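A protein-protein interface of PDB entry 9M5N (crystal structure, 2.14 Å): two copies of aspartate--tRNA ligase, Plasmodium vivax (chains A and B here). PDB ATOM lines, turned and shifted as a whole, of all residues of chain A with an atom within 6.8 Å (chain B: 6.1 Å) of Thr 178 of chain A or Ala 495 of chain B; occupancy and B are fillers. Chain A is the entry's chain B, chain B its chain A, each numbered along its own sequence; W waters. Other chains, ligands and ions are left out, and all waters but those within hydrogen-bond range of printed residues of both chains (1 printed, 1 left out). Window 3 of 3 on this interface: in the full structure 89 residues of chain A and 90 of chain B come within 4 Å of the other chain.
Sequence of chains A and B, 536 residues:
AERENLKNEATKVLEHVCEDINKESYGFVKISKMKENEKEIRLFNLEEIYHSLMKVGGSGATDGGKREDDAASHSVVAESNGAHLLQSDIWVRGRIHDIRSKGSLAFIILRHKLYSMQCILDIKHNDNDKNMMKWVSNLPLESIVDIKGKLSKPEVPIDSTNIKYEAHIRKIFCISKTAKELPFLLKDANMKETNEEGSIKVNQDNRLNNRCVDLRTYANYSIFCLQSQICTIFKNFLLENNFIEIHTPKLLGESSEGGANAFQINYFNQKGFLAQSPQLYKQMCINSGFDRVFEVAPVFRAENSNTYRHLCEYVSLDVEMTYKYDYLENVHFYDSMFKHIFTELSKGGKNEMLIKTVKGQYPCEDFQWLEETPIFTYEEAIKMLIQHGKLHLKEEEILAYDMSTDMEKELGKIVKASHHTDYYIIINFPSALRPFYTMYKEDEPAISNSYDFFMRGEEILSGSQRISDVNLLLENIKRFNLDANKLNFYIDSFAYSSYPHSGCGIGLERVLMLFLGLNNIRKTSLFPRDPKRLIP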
ATOM      1  N   PHE A  28      -2.584 -24.333  18.465  1.00  0.00           N
ATOM      2  CA  PHE A  28      -3.930 -23.918  18.106  1.00  0.00           C
ATOM      3  C   PHE A  28      -4.893 -24.357  19.195  1.00  0.00           C
ATOM      4  O   PHE A  28      -4.810 -25.479  19.703  1.00  0.00           O
ATOM      5  CB  PHE A  28      -4.336 -24.510  16.760  1.00  0.00           C
ATOM      6  CG  PHE A  28      -3.443 -24.091  15.634  1.00  0.00           C
ATOM      7  CD1 PHE A  28      -3.594 -22.843  15.046  1.00  0.00           C
ATOM      8  CD2 PHE A  28      -2.438 -24.930  15.178  1.00  0.00           C
ATOM      9  CE1 PHE A  28      -2.767 -22.440  14.015  1.00  0.00           C
ATOM     10  CE2 PHE A  28      -1.605 -24.537  14.145  1.00  0.00           C
ATOM     11  CZ  PHE A  28      -1.769 -23.288  13.563  1.00  0.00           C
ATOM     12  N   ILE A  96      -1.472 -11.092  13.688  1.00  0.00           N
ATOM     13  CA  ILE A  96      -0.053 -11.153  13.326  1.00  0.00           C
ATOM     14  C   ILE A  96       0.141 -10.304  12.077  1.00  0.00           C
ATOM     15  O   ILE A  96      -0.109 -10.760  10.955  1.00  0.00           O
ATOM     16  CB  ILE A  96       0.425 -12.600  13.113  1.00  0.00           C
ATOM     17  CG1 ILE A  96       0.277 -13.400  14.412  1.00  0.00           C
ATOM     18  CG2 ILE A  96       1.877 -12.629  12.649  1.00  0.00           C
ATOM     19  CD1 ILE A  96       0.862 -14.795  14.367  1.00  0.00           C
ATOM     20  N   PRO A 140       0.631 -18.194   9.765  1.00  0.00           N
ATOM     21  CA  PRO A 140       0.360 -17.286   8.639  1.00  0.00           C
ATOM     22  C   PRO A 140       0.021 -15.882   9.114  1.00  0.00           C
ATOM     23  O   PRO A 140      -0.593 -15.689  10.166  1.00  0.00           O
ATOM     24  CB  PRO A 140      -0.857 -17.916   7.942  1.00  0.00           C
ATOM     25  CG  PRO A 140      -1.099 -19.236   8.625  1.00  0.00           C
ATOM     26  CD  PRO A 140      -0.441 -19.180   9.969  1.00  0.00           C
ATOM     27  N   LEU A 141       0.398 -14.891   8.304  1.00  0.00           N
ATOM     28  CA  LEU A 141       0.051 -13.514   8.622  1.00  0.00           C
ATOM     29  C   LEU A 141      -1.464 -13.356   8.687  1.00  0.00           C
ATOM     30  O   LEU A 141      -2.216 -14.075   8.021  1.00  0.00           O
ATOM     31  CB  LEU A 141       0.638 -12.555   7.584  1.00  0.00           C
ATOM     32  CG  LEU A 141       2.168 -12.498   7.514  1.00  0.00           C
ATOM     33  CD1 LEU A 141       2.609 -11.421   6.549  1.00  0.00           C
ATOM     34  CD2 LEU A 141       2.771 -12.259   8.886  1.00  0.00           C
ATOM     35  N   GLU A 142      -1.898 -12.396   9.503  1.00  0.00           N
ATOM     36  CA  GLU A 142      -3.277 -12.027   9.821  1.00  0.00           C
ATOM     37  C   GLU A 142      -3.895 -12.981  10.825  1.00  0.00           C
ATOM     38  O   GLU A 142      -5.033 -12.737  11.268  1.00  0.00           O
ATOM     39  CB  GLU A 142      -4.199 -11.953   8.590  1.00  0.00           C
ATOM     40  CG  GLU A 142      -3.903 -10.789   7.676  1.00  0.00           C
ATOM     41  CD  GLU A 142      -3.846  -9.481   8.427  1.00  0.00           C
ATOM     42  OE1 GLU A 142      -2.725  -9.018   8.721  1.00  0.00           O
ATOM     43  OE2 GLU A 142      -4.919  -8.923   8.738  1.00  0.00           O
ATOM     44  N   SER A 143      -3.201 -14.054  11.206  1.00  0.00           N
ATOM     45  CA  SER A 143      -3.759 -14.967  12.188  1.00  0.00           C
ATOM     46  C   SER A 143      -3.978 -14.247  13.509  1.00  0.00           C
ATOM     47  O   SER A 143      -3.186 -13.390  13.910  1.00  0.00           O
ATOM     48  CB  SER A 143      -2.838 -16.166  12.389  1.00  0.00           C
ATOM     49  OG  SER A 143      -2.842 -17.002  11.250  1.00  0.00           O
ATOM     50  N   ILE A 144      -5.077 -14.580  14.167  1.00  0.00           N
ATOM     51  CA  ILE A 144      -5.402 -14.018  15.465  1.00  0.00           C
ATOM     52  C   ILE A 144      -4.841 -14.917  16.552  1.00  0.00           C
ATOM     53  O   ILE A 144      -5.084 -16.140  16.565  1.00  0.00           O
ATOM     54  CB  ILE A 144      -6.914 -13.837  15.641  1.00  0.00           C
ATOM     55  CG1 ILE A 144      -7.448 -12.822  14.622  1.00  0.00           C
ATOM     56  CG2 ILE A 144      -7.182 -13.371  17.053  1.00  0.00           C
ATOM     57  CD1 ILE A 144      -8.976 -12.802  14.492  1.00  0.00           C
ATOM     58  N   CYS A 174      -2.915 -19.641  19.045  1.00  0.00           N
ATOM     59  CA  CYS A 174      -3.594 -19.124  17.866  1.00  0.00           C
ATOM     60  C   CYS A 174      -5.062 -19.534  17.922  1.00  0.00           C
ATOM     61  O   CYS A 174      -5.391 -20.719  17.799  1.00  0.00           O
ATOM     62  CB  CYS A 174      -2.935 -19.628  16.586  1.00  0.00           C
ATOM     63  SG  CYS A 174      -3.835 -19.184  15.075  1.00  0.00           S
ATOM     64  N   SER A 176      -7.332 -18.095  15.763  1.00  0.00           N
ATOM     65  CA  SER A 176      -7.895 -18.072  14.411  1.00  0.00           C
ATOM     66  C   SER A 176      -6.759 -18.086  13.399  1.00  0.00           C
ATOM     67  O   SER A 176      -6.017 -17.107  13.292  1.00  0.00           O
ATOM     68  CB  SER A 176      -8.798 -16.852  14.212  1.00  0.00           C
ATOM     69  OG  SER A 176      -9.602 -16.995  13.056  1.00  0.00           O
ATOM     70  N   LYS A 177      -6.633 -19.177  12.646  1.00  0.00           N
ATOM     71  CA  LYS A 177      -5.570 -19.298  11.656  1.00  0.00           C
ATOM     72  C   LYS A 177      -6.058 -18.798  10.301  1.00  0.00           C
ATOM     73  O   LYS A 177      -7.157 -19.151   9.855  1.00  0.00           O
ATOM     74  CB  LYS A 177      -5.085 -20.744  11.548  1.00  0.00           C
ATOM     75  CG  LYS A 177      -3.959 -20.954  10.548  1.00  0.00           C
ATOM     76  CD  LYS A 177      -3.668 -22.446  10.343  1.00  0.00           C
ATOM     77  CE  LYS A 177      -3.799 -22.854   8.874  1.00  0.00           C
ATOM     78  NZ  LYS A 177      -3.830 -24.335   8.690  1.00  0.00           N
ATOM     79  N   THR A 178      -5.255 -17.943   9.669  1.00  0.00           N
ATOM     80  CA  THR A 178      -5.509 -17.558   8.290  1.00  0.00           C
ATOM     81  C   THR A 178      -5.573 -18.806   7.420  1.00  0.00           C
ATOM     82  O   THR A 178      -4.704 -19.678   7.502  1.00  0.00           O
ATOM     83  CB  THR A 178      -4.410 -16.617   7.801  1.00  0.00           C
ATOM     84  OG1 THR A 178      -4.364 -15.473   8.658  1.00  0.00           O
ATOM     85  CG2 THR A 178      -4.670 -16.165   6.366  1.00  0.00           C
ATOM     86  N   ALA A 179      -6.622 -18.902   6.611  1.00  0.00           N
ATOM     87  CA  ALA A 179      -6.887 -20.106   5.835  1.00  0.00           C
ATOM     88  C   ALA A 179      -6.492 -19.971   4.375  1.00  0.00           C
ATOM     89  O   ALA A 179      -6.189 -20.975   3.727  1.00  0.00           O
ATOM     90  CB  ALA A 179      -8.377 -20.470   5.921  1.00  0.00           C
ATOM     91  N   LYS A 180      -6.517 -18.753   3.850  1.00  0.00           N
ATOM     92  CA  LYS A 180      -6.252 -18.446   2.455  1.00  0.00           C
ATOM     93  C   LYS A 180      -5.085 -17.484   2.373  1.00  0.00           C
ATOM     94  O   LYS A 180      -4.968 -16.577   3.205  1.00  0.00           O
ATOM     95  CB  LYS A 180      -7.454 -17.775   1.785  1.00  0.00           C
ATOM     96  CG  LYS A 180      -8.437 -18.698   1.148  1.00  0.00           C
ATOM     97  CD  LYS A 180      -8.674 -18.325  -0.300  1.00  0.00           C
ATOM     98  CE  LYS A 180      -9.390 -17.013  -0.417  1.00  0.00           C
ATOM     99  NZ  LYS A 180      -9.777 -16.774  -1.834  1.00  0.00           N
ATOM    100  N   GLU A 181      -4.248 -17.652   1.352  1.00  0.00           N
ATOM    101  CA  GLU A 181      -3.298 -16.605   1.017  1.00  0.00           C
ATOM    102  C   GLU A 181      -4.039 -15.302   0.749  1.00  0.00           C
ATOM    103  O   GLU A 181      -5.055 -15.282   0.047  1.00  0.00           O
ATOM    104  CB  GLU A 181      -2.486 -16.991  -0.206  1.00  0.00           C
ATOM    105  CG  GLU A 181      -1.199 -16.217  -0.292  1.00  0.00           C
ATOM    106  CD  GLU A 181      -0.339 -16.673  -1.434  1.00  0.00           C
ATOM    107  OE1 GLU A 181       0.479 -17.596  -1.228  1.00  0.00           O
ATOM    108  OE2 GLU A 181      -0.500 -16.114  -2.543  1.00  0.00           O
ATOM    109  N   LEU A 182      -3.532 -14.212   1.311  1.00  0.00           N
ATOM    110  CA  LEU A 182      -4.185 -12.925   1.135  1.00  0.00           C
ATOM    111  C   LEU A 182      -4.224 -12.555  -0.348  1.00  0.00           C
ATOM    112  O   LEU A 182      -3.386 -13.014  -1.131  1.00  0.00           O
ATOM    113  CB  LEU A 182      -3.460 -11.854   1.952  1.00  0.00           C
ATOM    114  CG  LEU A 182      -4.074 -11.636   3.345  1.00  0.00           C
ATOM    115  CD1 LEU A 182      -4.040 -12.937   4.143  1.00  0.00           C
ATOM    116  CD2 LEU A 182      -3.372 -10.511   4.113  1.00  0.00           C
ATOM    117  N   ARG A 216      -8.064  -3.179   6.266  1.00  0.00           N
ATOM    118  CA  ARG A 216      -7.145  -3.396   7.375  1.00  0.00           C
ATOM    119  C   ARG A 216      -5.958  -2.443   7.367  1.00  0.00           C
ATOM    120  O   ARG A 216      -5.265  -2.349   8.390  1.00  0.00           O
ATOM    121  CB  ARG A 216      -6.655  -4.850   7.374  1.00  0.00           C
ATOM    122  CG  ARG A 216      -7.799  -5.842   7.535  1.00  0.00           C
ATOM    123  CD  ARG A 216      -7.353  -7.303   7.524  1.00  0.00           C
ATOM    124  NE  ARG A 216      -8.512  -8.177   7.357  1.00  0.00           N
ATOM    125  CZ  ARG A 216      -8.533  -9.474   7.637  1.00  0.00           C
ATOM    126  NH1 ARG A 216      -7.466 -10.096   8.127  1.00  0.00           N
ATOM    127  NH2 ARG A 216      -9.651 -10.166   7.415  1.00  0.00           N
ATOM    128  N   VAL B 470     -14.376 -20.370   9.137  1.00  0.00           N
ATOM    129  CA  VAL B 470     -14.865 -20.338   7.765  1.00  0.00           C
ATOM    130  C   VAL B 470     -15.282 -21.732   7.294  1.00  0.00           C
ATOM    131  O   VAL B 470     -16.229 -21.871   6.509  1.00  0.00           O
ATOM    132  CB  VAL B 470     -13.803 -19.683   6.858  1.00  0.00           C
ATOM    133  CG1 VAL B 470     -12.477 -20.381   7.009  1.00  0.00           C
ATOM    134  CG2 VAL B 470     -14.251 -19.683   5.415  1.00  0.00           C
ATOM    135  N   ILE B 491     -18.331 -15.032   2.569  1.00  0.00           N
ATOM    136  CA  ILE B 491     -17.582 -16.180   3.080  1.00  0.00           C
ATOM    137  C   ILE B 491     -16.095 -15.877   3.065  1.00  0.00           C
ATOM    138  O   ILE B 491     -15.377 -16.153   4.032  1.00  0.00           O
ATOM    139  CB  ILE B 491     -17.891 -17.450   2.264  1.00  0.00           C
ATOM    140  CG1 ILE B 491     -19.379 -17.796   2.310  1.00  0.00           C
ATOM    141  CG2 ILE B 491     -17.030 -18.627   2.739  1.00  0.00           C
ATOM    142  CD1 ILE B 491     -19.798 -18.703   1.155  1.00  0.00           C
ATOM    143  N   ASP B 492     -15.615 -15.309   1.961  1.00  0.00           N
ATOM    144  CA  ASP B 492     -14.205 -14.978   1.840  1.00  0.00           C
ATOM    145  C   ASP B 492     -13.730 -14.107   2.999  1.00  0.00           C
ATOM    146  O   ASP B 492     -12.588 -14.254   3.450  1.00  0.00           O
ATOM    147  CB  ASP B 492     -13.968 -14.294   0.493  1.00  0.00           C
ATOM    148  CG  ASP B 492     -12.511 -14.241   0.112  1.00  0.00           C
ATOM    149  OD1 ASP B 492     -11.934 -15.321  -0.150  1.00  0.00           O
ATOM    150  OD2 ASP B 492     -11.945 -13.120   0.069  1.00  0.00           O
ATOM    151  N   SER B 493     -14.600 -13.244   3.539  1.00  0.00           N
ATOM    152  CA  SER B 493     -14.135 -12.340   4.583  1.00  0.00           C
ATOM    153  C   SER B 493     -13.792 -13.070   5.875  1.00  0.00           C
ATOM    154  O   SER B 493     -13.176 -12.467   6.763  1.00  0.00           O
ATOM    155  CB  SER B 493     -15.177 -11.245   4.844  1.00  0.00           C
ATOM    156  OG  SER B 493     -16.279 -11.731   5.592  1.00  0.00           O
ATOM    157  N   PHE B 494     -14.144 -14.351   5.989  1.00  0.00           N
ATOM    158  CA  PHE B 494     -13.739 -15.177   7.124  1.00  0.00           C
ATOM    159  C   PHE B 494     -12.466 -15.967   6.855  1.00  0.00           C
ATOM    160  O   PHE B 494     -12.022 -16.709   7.735  1.00  0.00           O
ATOM    161  CB  PHE B 494     -14.862 -16.162   7.509  1.00  0.00           C
ATOM    162  CG  PHE B 494     -16.149 -15.503   7.924  1.00  0.00           C
ATOM    163  CD1 PHE B 494     -16.472 -15.368   9.266  1.00  0.00           C
ATOM    164  CD2 PHE B 494     -17.044 -15.029   6.972  1.00  0.00           C
ATOM    165  CE1 PHE B 494     -17.660 -14.772   9.655  1.00  0.00           C
ATOM    166  CE2 PHE B 494     -18.235 -14.428   7.354  1.00  0.00           C
ATOM    167  CZ  PHE B 494     -18.546 -14.304   8.695  1.00  0.00           C
ATOM    168  N   ALA B 495     -11.892 -15.858   5.658  1.00  0.00           N
ATOM    169  CA  ALA B 495     -10.801 -16.740   5.247  1.00  0.00           C
ATOM    170  C   ALA B 495      -9.416 -16.248   5.663  1.00  0.00           C
ATOM    171  O   ALA B 495      -8.441 -17.004   5.536  1.00  0.00           O
ATOM    172  CB  ALA B 495     -10.834 -16.936   3.728  1.00  0.00           C
ATOM    173  N   TYR B 496      -9.302 -15.016   6.159  1.00  0.00           N
ATOM    174  CA  TYR B 496      -8.034 -14.451   6.610  1.00  0.00           C
ATOM    175  C   TYR B 496      -8.131 -14.135   8.094  1.00  0.00           C
ATOM    176  O   TYR B 496      -7.706 -13.065   8.538  1.00  0.00           O
ATOM    177  CB  TYR B 496      -7.676 -13.211   5.786  1.00  0.00           C
ATOM    178  CG  TYR B 496      -8.084 -13.363   4.332  1.00  0.00           C
ATOM    179  CD1 TYR B 496      -7.329 -14.142   3.459  1.00  0.00           C
ATOM    180  CD2 TYR B 496      -9.239 -12.756   3.841  1.00  0.00           C
ATOM    181  CE1 TYR B 496      -7.702 -14.305   2.138  1.00  0.00           C
ATOM    182  CE2 TYR B 496      -9.627 -12.912   2.520  1.00  0.00           C
ATOM    183  CZ  TYR B 496      -8.852 -13.692   1.670  1.00  0.00           C
ATOM    184  OH  TYR B 496      -9.222 -13.858   0.350  1.00  0.00           O
ATOM    185  N   SER B 497      -8.695 -15.093   8.846  1.00  0.00           N
ATOM    186  CA  SER B 497      -8.923 -15.079  10.289  1.00  0.00           C
ATOM    187  C   SER B 497     -10.216 -14.345  10.613  1.00  0.00           C
ATOM    188  O   SER B 497     -10.655 -13.480   9.851  1.00  0.00           O
ATOM    189  CB  SER B 497      -7.759 -14.456  11.057  1.00  0.00           C
ATOM    190  OG  SER B 497      -7.752 -13.042  10.933  1.00  0.00           O
HETATM  191  O   HOH W   1     -10.608 -12.728   7.392  1.00  0.00           O
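Hydrophobic or aromatic side chains of chain B within 4 Å of the printed part of chain A: Ala 495 and Tyr 496. Printed residues of chain A that touch a printed residue of chain B: Glu 142, Ile 144, Ser 176, Thr 178, Ala 179, Lys 180, Glu 181, Leu 182 and Arg 216. Along chain A the printed residues that touch a printed residue of chain B span positions 142 to 216. Among the printed residues, Asp or Glu carboxylates within 4 Å of a Lys or Arg side-chain nitrogen of the other chain: Lys 180 of chain A with Asp 492 of chain B (3.1 Å).
Among the printed residues, pairs that only touch across the chains: Glu 142 of chain A with Tyr 496 of chain B, Ile 144 of chain A with Ser 497 of chain B, Ser 176 of chain A with Ser 497 of chain B, Thr 178 of chain A with Ala 495 of chain B, Thr 178 of chain A with Tyr 496 of chain B, Lys 180 of chain A with Tyr 496 of chain B, Glu 181 of chain A with Tyr 496 of chain B and Leu 182 of chain A with Tyr 496 of chain B.
The side-chain carboxylate (OD1) of Asp 492 of chain B is in salt-bridge range of the side-chain amino group (NZ) of Lys 180 of chain A (3.1 Å). The backbone NH (N) of Ala 179 of chain A is in hydrogen-bond range of the backbone carbonyl oxygen (O) of Ala 495 of chain B, at 2.8 Å. O of Ala 495 of chain B lies within hydrogen-bond range of N of Lys 180 of chain A (3.1 Å). The backbone carbonyl oxygen (O) of Tyr 496 of chain B lies within hydrogen-bond range of the guanidinium group (NH1) of Arg 216 of chain A. O of Glu 142 of chain A sits at hydrogen-bond distance from OG of Ser 497 of chain B, at 2.8 Å.
No position is printed for both chains.
The side-chain carboxylate of Asp 492 of chain B sits at hydrogen-bond distance from the side-chain hydroxyl of Tyr 496 of chain B. The backbone carbonyl oxygen (O) of Ile 96 of chain A lies within hydrogen-bond range of the backbone NH (N) of Glu 142 of chain A (2.8 Å). O of Leu 141 of chain A sits at hydrogen-bond distance from OG1 of Thr 178 of chain A (2.6 Å). The backbone NH (N) of Thr 178 of chain A lies within hydrogen-bond range of the side-chain hydroxyl (OG) of Ser 143 of chain A (3.0 Å). SG of Cys 174 of chain A lies close to O of Ile 144 of chain A (3.6 Å). The side-chain sulfur (SG) of Cys 174 of chain A is in hydrogen-bond range of the backbone carbonyl oxygen (O) of Ser 176 of chain A, 3.5 Å away.
Water W1 lies within hydrogen-bond range of the backbone carbonyl oxygen of Ser 497 of chain B (2.6 Å), the backbone carbonyl oxygen of Ser 493 of chain B (2.7 Å), the guanidinium group of Arg 216 of chain A (2.7 Å) and the backbone NH of Tyr 496 of chain B (2.9 Å).
Thr 178 of chain A touches just these residues of chain B: Ala 495 (3.9 Å) and Tyr 496 (3.8 Å). Of chain A, only Thr 178 (3.9 Å), Ala 179 (2.8 Å) and Lys 180 (3.1 Å) come within 4 Å of Ala 495 of chain B. Printed residues of chain B within 4 Å of Ser 176 of chain A: Ser 497 (3.4 Å). Printed residues of chain B within 4 Å of Glu 142 of chain A: Tyr 496 (3.7 Å) and Ser 497 (2.8 Å). Printed residues of chain B within 4 Å of Ile 144 of chain A: Ser 497. Phe 28 of chain A touches none of the printed residues of chain B. Ile 96 of chain A touches none of the printed residues of chain B. The nearest residue of chain A that does not touch Ala 495 of chain B is Lys 177 of chain A (5.0 Å). The nearest printed residue of chain B that does not touch Glu 181 of chain A is Ala 495 of chain B (6.0 Å).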
